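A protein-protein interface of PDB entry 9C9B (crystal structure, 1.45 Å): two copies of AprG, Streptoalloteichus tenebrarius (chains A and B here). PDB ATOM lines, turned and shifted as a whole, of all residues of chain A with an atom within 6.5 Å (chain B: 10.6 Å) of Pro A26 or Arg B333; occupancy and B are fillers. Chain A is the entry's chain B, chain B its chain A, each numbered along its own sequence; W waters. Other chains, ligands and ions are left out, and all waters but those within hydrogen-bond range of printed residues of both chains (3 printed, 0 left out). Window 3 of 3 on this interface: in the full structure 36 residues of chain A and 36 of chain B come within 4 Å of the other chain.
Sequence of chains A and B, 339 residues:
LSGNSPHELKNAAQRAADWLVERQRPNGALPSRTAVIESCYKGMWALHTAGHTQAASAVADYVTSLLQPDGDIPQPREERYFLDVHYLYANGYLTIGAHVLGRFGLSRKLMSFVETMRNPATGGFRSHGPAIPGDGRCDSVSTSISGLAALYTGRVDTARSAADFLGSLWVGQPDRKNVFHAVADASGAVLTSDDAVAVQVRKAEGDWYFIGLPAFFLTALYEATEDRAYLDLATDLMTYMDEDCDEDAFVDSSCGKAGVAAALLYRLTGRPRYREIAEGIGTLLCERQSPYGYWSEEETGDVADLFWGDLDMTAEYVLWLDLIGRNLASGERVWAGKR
Printed residues of chain B that touch a printed residue of chain A: Pro B6, Gly B325, Arg B326, Ser B330 and Arg B333. Hydrophobic or aromatic side chains of chain B within 4 Å of the printed part of chain A: Pro B6. Along chain B the printed residues that touch a printed residue of chain A span positions 6 to 333. Printed residues of chain A that touch a printed residue of chain B: Pro A26, Gln A54, Ser A57, Ala A58 and Asp A61. Hydrophobic or aromatic side chains of chain A within 4 Å of the printed part of chain B: Ala A58. Among the printed residues, 9 pairs touch across the chains. Among the printed residues, Asp or Glu carboxylates within 4 Å of a Lys or Arg side-chain nitrogen of the other chain: Asp A61 with Arg B333 (2.8 Å).
O of Pro B6 sits at hydrogen-bond distance from NE2 of Gln A54 (3.0 Å). The side-chain hydroxyl of Ser B330 is in hydrogen-bond range of the side-chain carboxylate of Asp A61 (2.7 Å). The guanidinium group (NE) of Arg B333 sits at hydrogen-bond distance from the backbone carbonyl oxygen (O) of Pro A26 (2.9 Å). The guanidinium group of Arg B333 lies within salt-bridge range of the side-chain carboxylate of Asp A61.
Among the printed residues, merely in contact across the chains: Gln A54 with Gly B325 (3.6 Å), Gln A54 with Arg B326 (3.6 Å), Ser A57 with Arg B326 (3.6 Å), Ser A57 with Ser B330 (3.4 Å) and Ala A58 with Arg B333 (3.5 Å).
O of Arg B326 lies close to OG of Ser B330, at 3.4 Å.
No position is printed for both chains.
Of the printed residues of chain B, Pro A26 touches Arg B333. Of the printed residues of chain A, Arg B333 touches Pro A26 (2.9 Å), Ala A58 (3.5 Å) and Asp A61 (2.8 Å). Of chain B, only Arg B333 (3.5 Å) comes within 4 Å of Ala A58. Of the printed residues of chain B, Asp A61 touches Ser B330 and Arg B333. Of the printed residues of chain A, Pro B6 touches Gln A54 (3.0 Å). Of the printed residues of chain B, Ser A57 touches Arg B326 and Ser B330. Printed residues of chain B within 4 Å of Gln A54: Pro B6 (3.0 Å), Gly B325 (3.6 Å) and Arg B326 (3.6 Å). Printed residues of chain A within 4 Å of Ser B330: Ser A57 (3.4 Å) and Asp A61 (2.7 Å). Ala B263 touches none of the printed residues of chain A. The nearest printed residue of chain A that does not touch Gly B325 is Ser A57 (7.1 Å).
Water W1 lies within hydrogen-bond range of the side-chain amide nitrogen (NE2) of Gln A54 (2.9 Å) and the backbone NH (N) of Arg B326 (3.4 Å). Water W3 lies within hydrogen-bond range of the backbone carbonyl oxygen (O) of Gln A54 (2.9 Å), the side-chain hydroxyl (OG) of Ser B330 (3.0 Å) and the guanidinium group (NH2) of Arg B333 (3.1 Å). Water W2 lies within hydrogen-bond range of O of Arg A25 (2.9 Å) and NH1 of Arg B333 (3.2 Å).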
ATOM      1  N   GLN A  24     -16.579 -10.562 -23.834  1.00  0.00           N
ATOM      2  CA  GLN A  24     -17.456  -9.412 -23.998  1.00  0.00           C
ATOM      3  C   GLN A  24     -16.760  -8.149 -23.505  1.00  0.00           C
ATOM      4  O   GLN A  24     -16.011  -8.176 -22.527  1.00  0.00           O
ATOM      5  CB  GLN A  24     -18.746  -9.635 -23.211  1.00  0.00           C
ATOM      6  CG  GLN A  24     -19.796  -8.539 -23.423  1.00  0.00           C
ATOM      7  CD  GLN A  24     -21.126  -8.881 -22.773  1.00  0.00           C
ATOM      8  OE1 GLN A  24     -21.170  -9.529 -21.728  1.00  0.00           O
ATOM      9  NE2 GLN A  24     -22.209  -8.452 -23.389  1.00  0.00           N
ATOM     10  N   ARG A  25     -17.012  -7.039 -24.194  1.00  0.00           N
ATOM     11  CA  ARG A  25     -16.360  -5.778 -23.904  1.00  0.00           C
ATOM     12  C   ARG A  25     -17.110  -5.024 -22.809  1.00  0.00           C
ATOM     13  O   ARG A  25     -18.280  -5.303 -22.534  1.00  0.00           O
ATOM     14  CB  ARG A  25     -16.275  -4.957 -25.190  1.00  0.00           C
ATOM     15  CG  ARG A  25     -15.757  -5.795 -26.358  1.00  0.00           C
ATOM     16  CD  ARG A  25     -14.974  -4.994 -27.376  1.00  0.00           C
ATOM     17  NE  ARG A  25     -14.141  -5.857 -28.213  1.00  0.00           N
ATOM     18  CZ  ARG A  25     -14.337  -6.061 -29.512  1.00  0.00           C
ATOM     19  NH1 ARG A  25     -15.348  -5.469 -30.134  1.00  0.00           N
ATOM     20  NH2 ARG A  25     -13.523  -6.861 -30.192  1.00  0.00           N
ATOM     21  N   PRO A  26     -16.443  -4.076 -22.143  1.00  0.00           N
ATOM     22  CA  PRO A  26     -17.102  -3.369 -21.029  1.00  0.00           C
ATOM     23  C   PRO A  26     -18.412  -2.693 -21.400  1.00  0.00           C
ATOM     24  O   PRO A  26     -19.346  -2.684 -20.587  1.00  0.00           O
ATOM     25  CB  PRO A  26     -16.028  -2.372 -20.567  1.00  0.00           C
ATOM     26  CG  PRO A  26     -14.734  -3.047 -20.935  1.00  0.00           C
ATOM     27  CD  PRO A  26     -15.001  -3.774 -22.219  1.00  0.00           C
ATOM     28  N   ASN A  27     -18.518  -2.138 -22.604  1.00  0.00           N
ATOM     29  CA  ASN A  27     -19.763  -1.516 -23.032  1.00  0.00           C
ATOM     30  C   ASN A  27     -20.827  -2.528 -23.444  1.00  0.00           C
ATOM     31  O   ASN A  27     -21.951  -2.128 -23.759  1.00  0.00           O
ATOM     32  CB  ASN A  27     -19.503  -0.515 -24.167  1.00  0.00           C
ATOM     33  CG  ASN A  27     -19.147  -1.187 -25.485  1.00  0.00           C
ATOM     34  OD1 ASN A  27     -18.719  -2.344 -25.515  1.00  0.00           O
ATOM     35  ND2 ASN A  27     -19.303  -0.450 -26.585  1.00  0.00           N
ATOM     36  N   GLY A  28     -20.509  -3.819 -23.435  1.00  0.00           N
ATOM     37  CA  GLY A  28     -21.458  -4.847 -23.807  1.00  0.00           C
ATOM     38  C   GLY A  28     -21.288  -5.423 -25.202  1.00  0.00           C
ATOM     39  O   GLY A  28     -21.934  -6.431 -25.518  1.00  0.00           O
ATOM     40  N   ALA A  29     -20.457  -4.824 -26.052  1.00  0.00           N
ATOM     41  CA  ALA A  29     -20.302  -5.359 -27.398  1.00  0.00           C
ATOM     42  C   ALA A  29     -19.587  -6.710 -27.364  1.00  0.00           C
ATOM     43  O   ALA A  29     -18.783  -6.995 -26.472  1.00  0.00           O
ATOM     44  CB  ALA A  29     -19.535  -4.374 -28.282  1.00  0.00           C
ATOM     45  N   GLN A  54     -26.869 -11.302 -17.521  1.00  0.00           N
ATOM     46  CA  GLN A  54     -26.120 -10.056 -17.352  1.00  0.00           C
ATOM     47  C   GLN A  54     -25.390  -9.687 -18.637  1.00  0.00           C
ATOM     48  O   GLN A  54     -25.399  -8.522 -19.049  1.00  0.00           O
ATOM     49  CB  GLN A  54     -25.181 -10.145 -16.149  1.00  0.00           C
ATOM     50  CG  GLN A  54     -25.924  -9.879 -14.849  1.00  0.00           C
ATOM     51  CD  GLN A  54     -25.162 -10.295 -13.609  1.00  0.00           C
ATOM     52  OE1 GLN A  54     -23.955 -10.070 -13.494  1.00  0.00           O
ATOM     53  NE2 GLN A  54     -25.876 -10.903 -12.662  1.00  0.00           N
ATOM     54  N   SER A  57     -28.064  -8.508 -21.050  1.00  0.00           N
ATOM     55  CA  SER A  57     -28.463  -7.147 -20.717  1.00  0.00           C
ATOM     56  C   SER A  57     -27.392  -6.138 -21.106  1.00  0.00           C
ATOM     57  O   SER A  57     -27.720  -5.006 -21.490  1.00  0.00           O
ATOM     58  CB  SER A  57     -28.763  -7.066 -19.223  1.00  0.00           C
ATOM     59  OG  SER A  57     -29.854  -7.901 -18.894  1.00  0.00           O
ATOM     60  N   ALA A  58     -26.117  -6.524 -21.024  1.00  0.00           N
ATOM     61  CA  ALA A  58     -25.042  -5.643 -21.464  1.00  0.00           C
ATOM     62  C   ALA A  58     -25.105  -5.406 -22.968  1.00  0.00           C
ATOM     63  O   ALA A  58     -24.899  -4.277 -23.431  1.00  0.00           O
ATOM     64  CB  ALA A  58     -23.686  -6.208 -21.047  1.00  0.00           C
ATOM     65  N   VAL A  59     -25.405  -6.447 -23.752  1.00  0.00           N
ATOM     66  CA  VAL A  59     -25.657  -6.215 -25.174  1.00  0.00           C
ATOM     67  C   VAL A  59     -26.835  -5.263 -25.353  1.00  0.00           C
ATOM     68  O   VAL A  59     -26.802  -4.370 -26.208  1.00  0.00           O
ATOM     69  CB  VAL A  59     -25.855  -7.532 -25.950  1.00  0.00           C
ATOM     70  CG1 VAL A  59     -26.117  -7.236 -27.428  1.00  0.00           C
ATOM     71  CG2 VAL A  59     -24.642  -8.459 -25.790  1.00  0.00           C
ATOM     72  N   ASP A  61     -27.690  -2.874 -23.361  1.00  0.00           N
ATOM     73  CA  ASP A  61     -27.188  -1.532 -23.078  1.00  0.00           C
ATOM     74  C   ASP A  61     -26.470  -0.958 -24.292  1.00  0.00           C
ATOM     75  O   ASP A  61     -26.650   0.223 -24.633  1.00  0.00           O
ATOM     76  CB  ASP A  61     -26.244  -1.572 -21.871  1.00  0.00           C
ATOM     77  CG  ASP A  61     -26.928  -2.037 -20.592  1.00  0.00           C
ATOM     78  OD1 ASP A  61     -28.140  -1.768 -20.428  1.00  0.00           O
ATOM     79  OD2 ASP A  61     -26.239  -2.649 -19.738  1.00  0.00           O
ATOM     80  N   TYR A  62     -25.649  -1.779 -24.953  1.00  0.00           N
ATOM     81  CA  TYR A  62     -24.933  -1.341 -26.149  1.00  0.00           C
ATOM     82  C   TYR A  62     -25.909  -0.984 -27.262  1.00  0.00           C
ATOM     83  O   TYR A  62     -25.815   0.087 -27.876  1.00  0.00           O
ATOM     84  CB  TYR A  62     -23.971  -2.449 -26.593  1.00  0.00           C
ATOM     85  CG  TYR A  62     -23.298  -2.192 -27.924  1.00  0.00           C
ATOM     86  CD1 TYR A  62     -22.516  -1.061 -28.105  1.00  0.00           C
ATOM     87  CD2 TYR A  62     -23.422  -3.083 -28.985  1.00  0.00           C
ATOM     88  CE1 TYR A  62     -21.894  -0.807 -29.304  1.00  0.00           C
ATOM     89  CE2 TYR A  62     -22.793  -2.836 -30.199  1.00  0.00           C
ATOM     90  CZ  TYR A  62     -22.029  -1.697 -30.346  1.00  0.00           C
ATOM     91  OH  TYR A  62     -21.398  -1.419 -31.543  1.00  0.00           O
ATOM     92  N   PRO B   6     -23.318  -8.404  -8.494  1.00  0.00           N
ATOM     93  CA  PRO B   6     -24.252  -9.066  -9.421  1.00  0.00           C
ATOM     94  C   PRO B   6     -23.811 -10.462  -9.829  1.00  0.00           C
ATOM     95  O   PRO B   6     -24.654 -11.361  -9.943  1.00  0.00           O
ATOM     96  CB  PRO B   6     -24.292  -8.097 -10.613  1.00  0.00           C
ATOM     97  CG  PRO B   6     -24.014  -6.775 -10.004  1.00  0.00           C
ATOM     98  CD  PRO B   6     -22.992  -7.035  -8.934  1.00  0.00           C
ATOM     99  N   ALA B 263     -34.308  -2.653  -8.152  1.00  0.00           N
ATOM    100  CA  ALA B 263     -33.215  -2.818  -9.104  1.00  0.00           C
ATOM    101  C   ALA B 263     -33.588  -2.237 -10.462  1.00  0.00           C
ATOM    102  O   ALA B 263     -32.775  -1.557 -11.102  1.00  0.00           O
ATOM    103  CB  ALA B 263     -32.845  -4.297  -9.221  1.00  0.00           C
ATOM    104  N   TYR B 266     -33.654   1.511 -10.257  1.00  0.00           N
ATOM    105  CA  TYR B 266     -32.283   2.008 -10.310  1.00  0.00           C
ATOM    106  C   TYR B 266     -31.771   2.080 -11.745  1.00  0.00           C
ATOM    107  O   TYR B 266     -31.220   3.105 -12.166  1.00  0.00           O
ATOM    108  CB  TYR B 266     -31.346   1.171  -9.429  1.00  0.00           C
ATOM    109  CG  TYR B 266     -29.892   1.589  -9.587  1.00  0.00           C
ATOM    110  CD1 TYR B 266     -29.473   2.864  -9.206  1.00  0.00           C
ATOM    111  CD2 TYR B 266     -28.947   0.723 -10.119  1.00  0.00           C
ATOM    112  CE1 TYR B 266     -28.155   3.253  -9.360  1.00  0.00           C
ATOM    113  CE2 TYR B 266     -27.623   1.103 -10.267  1.00  0.00           C
ATOM    114  CZ  TYR B 266     -27.236   2.374  -9.892  1.00  0.00           C
ATOM    115  OH  TYR B 266     -25.916   2.743 -10.048  1.00  0.00           O
ATOM    116  N   ARG B 267     -31.959   1.011 -12.525  1.00  0.00           N
ATOM    117  CA  ARG B 267     -31.511   1.064 -13.912  1.00  0.00           C
ATOM    118  C   ARG B 267     -32.183   2.203 -14.667  1.00  0.00           C
ATOM    119  O   ARG B 267     -31.539   2.889 -15.467  1.00  0.00           O
ATOM    120  CB  ARG B 267     -31.766  -0.257 -14.633  1.00  0.00           C
ATOM    121  CG  ARG B 267     -31.406  -0.143 -16.094  1.00  0.00           C
ATOM    122  CD  ARG B 267     -31.310  -1.466 -16.796  1.00  0.00           C
ATOM    123  NE  ARG B 267     -32.557  -2.222 -16.816  1.00  0.00           N
ATOM    124  CZ  ARG B 267     -33.567  -2.018 -17.658  1.00  0.00           C
ATOM    125  NH1 ARG B 267     -33.515  -1.064 -18.575  1.00  0.00           N
ATOM    126  NH2 ARG B 267     -34.635  -2.798 -17.585  1.00  0.00           N
ATOM    127  N   LEU B 268     -33.468   2.434 -14.407  1.00  0.00           N
ATOM    128  CA  LEU B 268     -34.214   3.421 -15.183  1.00  0.00           C
ATOM    129  C   LEU B 268     -33.945   4.855 -14.728  1.00  0.00           C
ATOM    130  O   LEU B 268     -33.975   5.775 -15.555  1.00  0.00           O
ATOM    131  CB  LEU B 268     -35.710   3.123 -15.111  1.00  0.00           C
ATOM    132  CG  LEU B 268     -36.114   1.783 -15.726  1.00  0.00           C
ATOM    133  CD1 LEU B 268     -37.613   1.610 -15.600  1.00  0.00           C
ATOM    134  CD2 LEU B 268     -35.693   1.715 -17.176  1.00  0.00           C
ATOM    135  N   GLY B 270     -31.455   5.789 -11.908  1.00  0.00           N
ATOM    136  CA  GLY B 270     -30.181   6.040 -11.275  1.00  0.00           C
ATOM    137  C   GLY B 270     -30.239   6.454  -9.820  1.00  0.00           C
ATOM    138  O   GLY B 270     -29.182   6.735  -9.241  1.00  0.00           O
ATOM    139  N   ARG B 275     -30.688   1.448  -5.700  1.00  0.00           N
ATOM    140  CA  ARG B 275     -29.545   0.539  -5.720  1.00  0.00           C
ATOM    141  C   ARG B 275     -29.323  -0.081  -4.349  1.00  0.00           C
ATOM    142  O   ARG B 275     -29.126  -1.295  -4.233  1.00  0.00           O
ATOM    143  CB  ARG B 275     -28.275   1.254  -6.191  1.00  0.00           C
ATOM    144  CG  ARG B 275     -27.043   0.342  -6.202  1.00  0.00           C
ATOM    145  CD  ARG B 275     -25.723   1.096  -6.402  1.00  0.00           C
ATOM    146  NE  ARG B 275     -25.637   2.365  -5.677  1.00  0.00           N
ATOM    147  CZ  ARG B 275     -25.385   2.493  -4.376  1.00  0.00           C
ATOM    148  NH1 ARG B 275     -25.190   1.425  -3.607  1.00  0.00           N
ATOM    149  NH2 ARG B 275     -25.326   3.703  -3.838  1.00  0.00           N
ATOM    150  N   GLU B 279     -29.552  -3.999  -3.592  1.00  0.00           N
ATOM    151  CA  GLU B 279     -28.332  -4.667  -3.130  1.00  0.00           C
ATOM    152  C   GLU B 279     -28.561  -5.381  -1.801  1.00  0.00           C
ATOM    153  O   GLU B 279     -28.135  -6.529  -1.624  1.00  0.00           O
ATOM    154  CB  GLU B 279     -27.195  -3.647  -2.989  1.00  0.00           C
ATOM    155  CG  GLU B 279     -26.454  -3.343  -4.282  1.00  0.00           C
ATOM    156  CD  GLU B 279     -25.394  -2.262  -4.122  1.00  0.00           C
ATOM    157  OE1 GLU B 279     -24.685  -1.971  -5.109  1.00  0.00           O
ATOM    158  OE2 GLU B 279     -25.276  -1.693  -3.016  1.00  0.00           O
ATOM    159  N   GLY B 325     -29.720  -8.937 -10.209  1.00  0.00           N
ATOM    160  CA  GLY B 325     -28.349  -8.885 -10.682  1.00  0.00           C
ATOM    161  C   GLY B 325     -28.210  -8.196 -12.025  1.00  0.00           C
ATOM    162  O   GLY B 325     -27.315  -7.371 -12.222  1.00  0.00           O
ATOM    163  N   ARG B 326     -29.084  -8.525 -12.976  1.00  0.00           N
ATOM    164  CA  ARG B 326     -28.908  -7.932 -14.298  1.00  0.00           C
ATOM    165  C   ARG B 326     -29.266  -6.451 -14.313  1.00  0.00           C
ATOM    166  O   ARG B 326     -28.626  -5.669 -15.021  1.00  0.00           O
ATOM    167  CB  ARG B 326     -29.628  -8.731 -15.372  1.00  0.00           C
ATOM    168  CG  ARG B 326     -31.115  -8.635 -15.384  1.00  0.00           C
ATOM    169  CD  ARG B 326     -31.597  -9.841 -16.164  1.00  0.00           C
ATOM    170  NE  ARG B 326     -32.876  -9.622 -16.798  1.00  0.00           N
ATOM    171  CZ  ARG B 326     -33.695 -10.605 -17.163  1.00  0.00           C
ATOM    172  NH1 ARG B 326     -33.384 -11.872 -16.915  1.00  0.00           N
ATOM    173  NH2 ARG B 326     -34.839 -10.313 -17.755  1.00  0.00           N
ATOM    174  N   ASN B 327     -30.265  -6.039 -13.527  1.00  0.00           N
ATOM    175  CA  ASN B 327     -30.581  -4.616 -13.461  1.00  0.00           C
ATOM    176  C   ASN B 327     -29.547  -3.820 -12.678  1.00  0.00           C
ATOM    177  O   ASN B 327     -29.265  -2.670 -13.042  1.00  0.00           O
ATOM    178  CB  ASN B 327     -32.005  -4.397 -12.966  1.00  0.00           C
ATOM    179  CG  ASN B 327     -33.028  -4.723 -14.036  1.00  0.00           C
ATOM    180  OD1 ASN B 327     -33.094  -4.050 -15.057  1.00  0.00           O
ATOM    181  ND2 ASN B 327     -33.812  -5.771 -13.820  1.00  0.00           N
ATOM    182  N   LEU B 328     -28.965  -4.400 -11.619  1.00  0.00           N
ATOM    183  CA  LEU B 328     -27.883  -3.713 -10.921  1.00  0.00           C
ATOM    184  C   LEU B 328     -26.657  -3.566 -11.812  1.00  0.00           C
ATOM    185  O   LEU B 328     -26.034  -2.497 -11.843  1.00  0.00           O
ATOM    186  CB  LEU B 328     -27.520  -4.449  -9.628  1.00  0.00           C
ATOM    187  CG  LEU B 328     -28.523  -4.274  -8.493  1.00  0.00           C
ATOM    188  CD1 LEU B 328     -28.056  -5.024  -7.253  1.00  0.00           C
ATOM    189  CD2 LEU B 328     -28.734  -2.795  -8.182  1.00  0.00           C
ATOM    190  N   ALA B 329     -26.304  -4.619 -12.553  1.00  0.00           N
ATOM    191  CA  ALA B 329     -25.136  -4.561 -13.427  1.00  0.00           C
ATOM    192  C   ALA B 329     -25.339  -3.544 -14.542  1.00  0.00           C
ATOM    193  O   ALA B 329     -24.450  -2.726 -14.812  1.00  0.00           O
ATOM    194  CB  ALA B 329     -24.830  -5.943 -14.005  1.00  0.00           C
ATOM    195  N   SER B 330     -26.504  -3.571 -15.196  1.00  0.00           N
ATOM    196  CA  SER B 330     -26.759  -2.593 -16.249  1.00  0.00           C
ATOM    197  C   SER B 330     -26.915  -1.191 -15.677  1.00  0.00           C
ATOM    198  O   SER B 330     -26.495  -0.210 -16.309  1.00  0.00           O
ATOM    199  CB  SER B 330     -27.989  -2.993 -17.068  1.00  0.00           C
ATOM    200  OG  SER B 330     -27.694  -4.082 -17.933  1.00  0.00           O
ATOM    201  N   GLY B 331     -27.514  -1.071 -14.489  1.00  0.00           N
ATOM    202  CA  GLY B 331     -27.627   0.241 -13.861  1.00  0.00           C
ATOM    203  C   GLY B 331     -26.275   0.846 -13.562  1.00  0.00           C
ATOM    204  O   GLY B 331     -26.059   2.043 -13.777  1.00  0.00           O
ATOM    205  N   GLU B 332     -25.332   0.028 -13.084  1.00  0.00           N
ATOM    206  CA  GLU B 332     -23.978   0.510 -12.850  1.00  0.00           C
ATOM    207  C   GLU B 332     -23.336   0.992 -14.149  1.00  0.00           C
ATOM    208  O   GLU B 332     -22.708   2.056 -14.187  1.00  0.00           O
ATOM    209  CB  GLU B 332     -23.143  -0.603 -12.218  1.00  0.00           C
ATOM    210  CG  GLU B 332     -22.803  -0.400 -10.749  1.00  0.00           C
ATOM    211  CD  GLU B 332     -24.024  -0.173  -9.873  1.00  0.00           C
ATOM    212  OE1 GLU B 332     -24.222   0.987  -9.439  1.00  0.00           O
ATOM    213  OE2 GLU B 332     -24.767  -1.153  -9.608  1.00  0.00           O
ATOM    214  N   ARG B 333     -23.495   0.218 -15.228  1.00  0.00           N
ATOM    215  CA  ARG B 333     -22.933   0.619 -16.516  1.00  0.00           C
ATOM    216  C   ARG B 333     -23.492   1.960 -16.963  1.00  0.00           C
ATOM    217  O   ARG B 333     -22.751   2.816 -17.468  1.00  0.00           O
ATOM    218  CB  ARG B 333     -23.224  -0.460 -17.564  1.00  0.00           C
ATOM    219  CG  ARG B 333     -22.729  -0.136 -18.975  1.00  0.00           C
ATOM    220  CD  ARG B 333     -22.951  -1.318 -19.951  1.00  0.00           C
ATOM    221  NE  ARG B 333     -22.114  -2.465 -19.617  1.00  0.00           N
ATOM    222  CZ  ARG B 333     -22.542  -3.553 -18.988  1.00  0.00           C
ATOM    223  NH1 ARG B 333     -21.689  -4.528 -18.697  1.00  0.00           N
ATOM    224  NH2 ARG B 333     -23.816  -3.669 -18.639  1.00  0.00           N
ATOM    225  N   VAL B 334     -24.793   2.175 -16.762  1.00  0.00           N
ATOM    226  CA  VAL B 334     -25.436   3.383 -17.267  1.00  0.00           C
ATOM    227  C   VAL B 334     -25.128   4.589 -16.379  1.00  0.00           C
ATOM    228  O   VAL B 334     -24.838   5.683 -16.881  1.00  0.00           O
ATOM    229  CB  VAL B 334     -26.951   3.147 -17.434  1.00  0.00           C
ATOM    230  CG1 VAL B 334     -27.690   4.464 -17.654  1.00  0.00           C
ATOM    231  CG2 VAL B 334     -27.225   2.141 -18.564  1.00  0.00           C
ATOM    232  N   TRP B 335     -25.159   4.416 -15.053  1.00  0.00           N
ATOM    233  CA  TRP B 335     -25.192   5.538 -14.120  1.00  0.00           C
ATOM    234  C   TRP B 335     -23.916   5.751 -13.318  1.00  0.00           C
ATOM    235  O   TRP B 335     -23.734   6.844 -12.774  1.00  0.00           O
ATOM    236  CB  TRP B 335     -26.339   5.367 -13.112  1.00  0.00           C
ATOM    237  CG  TRP B 335     -27.681   5.385 -13.719  1.00  0.00           C
ATOM    238  CD1 TRP B 335     -28.490   4.310 -13.951  1.00  0.00           C
ATOM    239  CD2 TRP B 335     -28.383   6.530 -14.204  1.00  0.00           C
ATOM    240  NE1 TRP B 335     -29.660   4.717 -14.539  1.00  0.00           N
ATOM    241  CE2 TRP B 335     -29.619   6.076 -14.711  1.00  0.00           C
ATOM    242  CE3 TRP B 335     -28.090   7.896 -14.259  1.00  0.00           C
ATOM    243  CZ2 TRP B 335     -30.563   6.937 -15.256  1.00  0.00           C
ATOM    244  CZ3 TRP B 335     -29.024   8.748 -14.803  1.00  0.00           C
ATOM    245  CH2 TRP B 335     -30.249   8.271 -15.297  1.00  0.00           C
ATOM    246  N   ALA B 336     -23.056   4.747 -13.198  1.00  0.00           N
ATOM    247  CA  ALA B 336     -21.890   4.859 -12.321  1.00  0.00           C
ATOM    248  C   ALA B 336     -20.595   5.092 -13.096  1.00  0.00           C
ATOM    249  O   ALA B 336     -20.525   4.853 -14.300  1.00  0.00           O
ATOM    250  CB  ALA B 336     -21.769   3.625 -11.427  1.00  0.00           C
HETATM  251  O   HOH W   1     -28.414 -11.813 -13.681  1.00  0.00           O
HETATM  252  O   HOH W   2     -19.348  -6.269 -19.993  1.00  0.00           O
HETATM  253  O   HOH W   3     -25.461  -6.076 -17.508  1.00  0.00           O
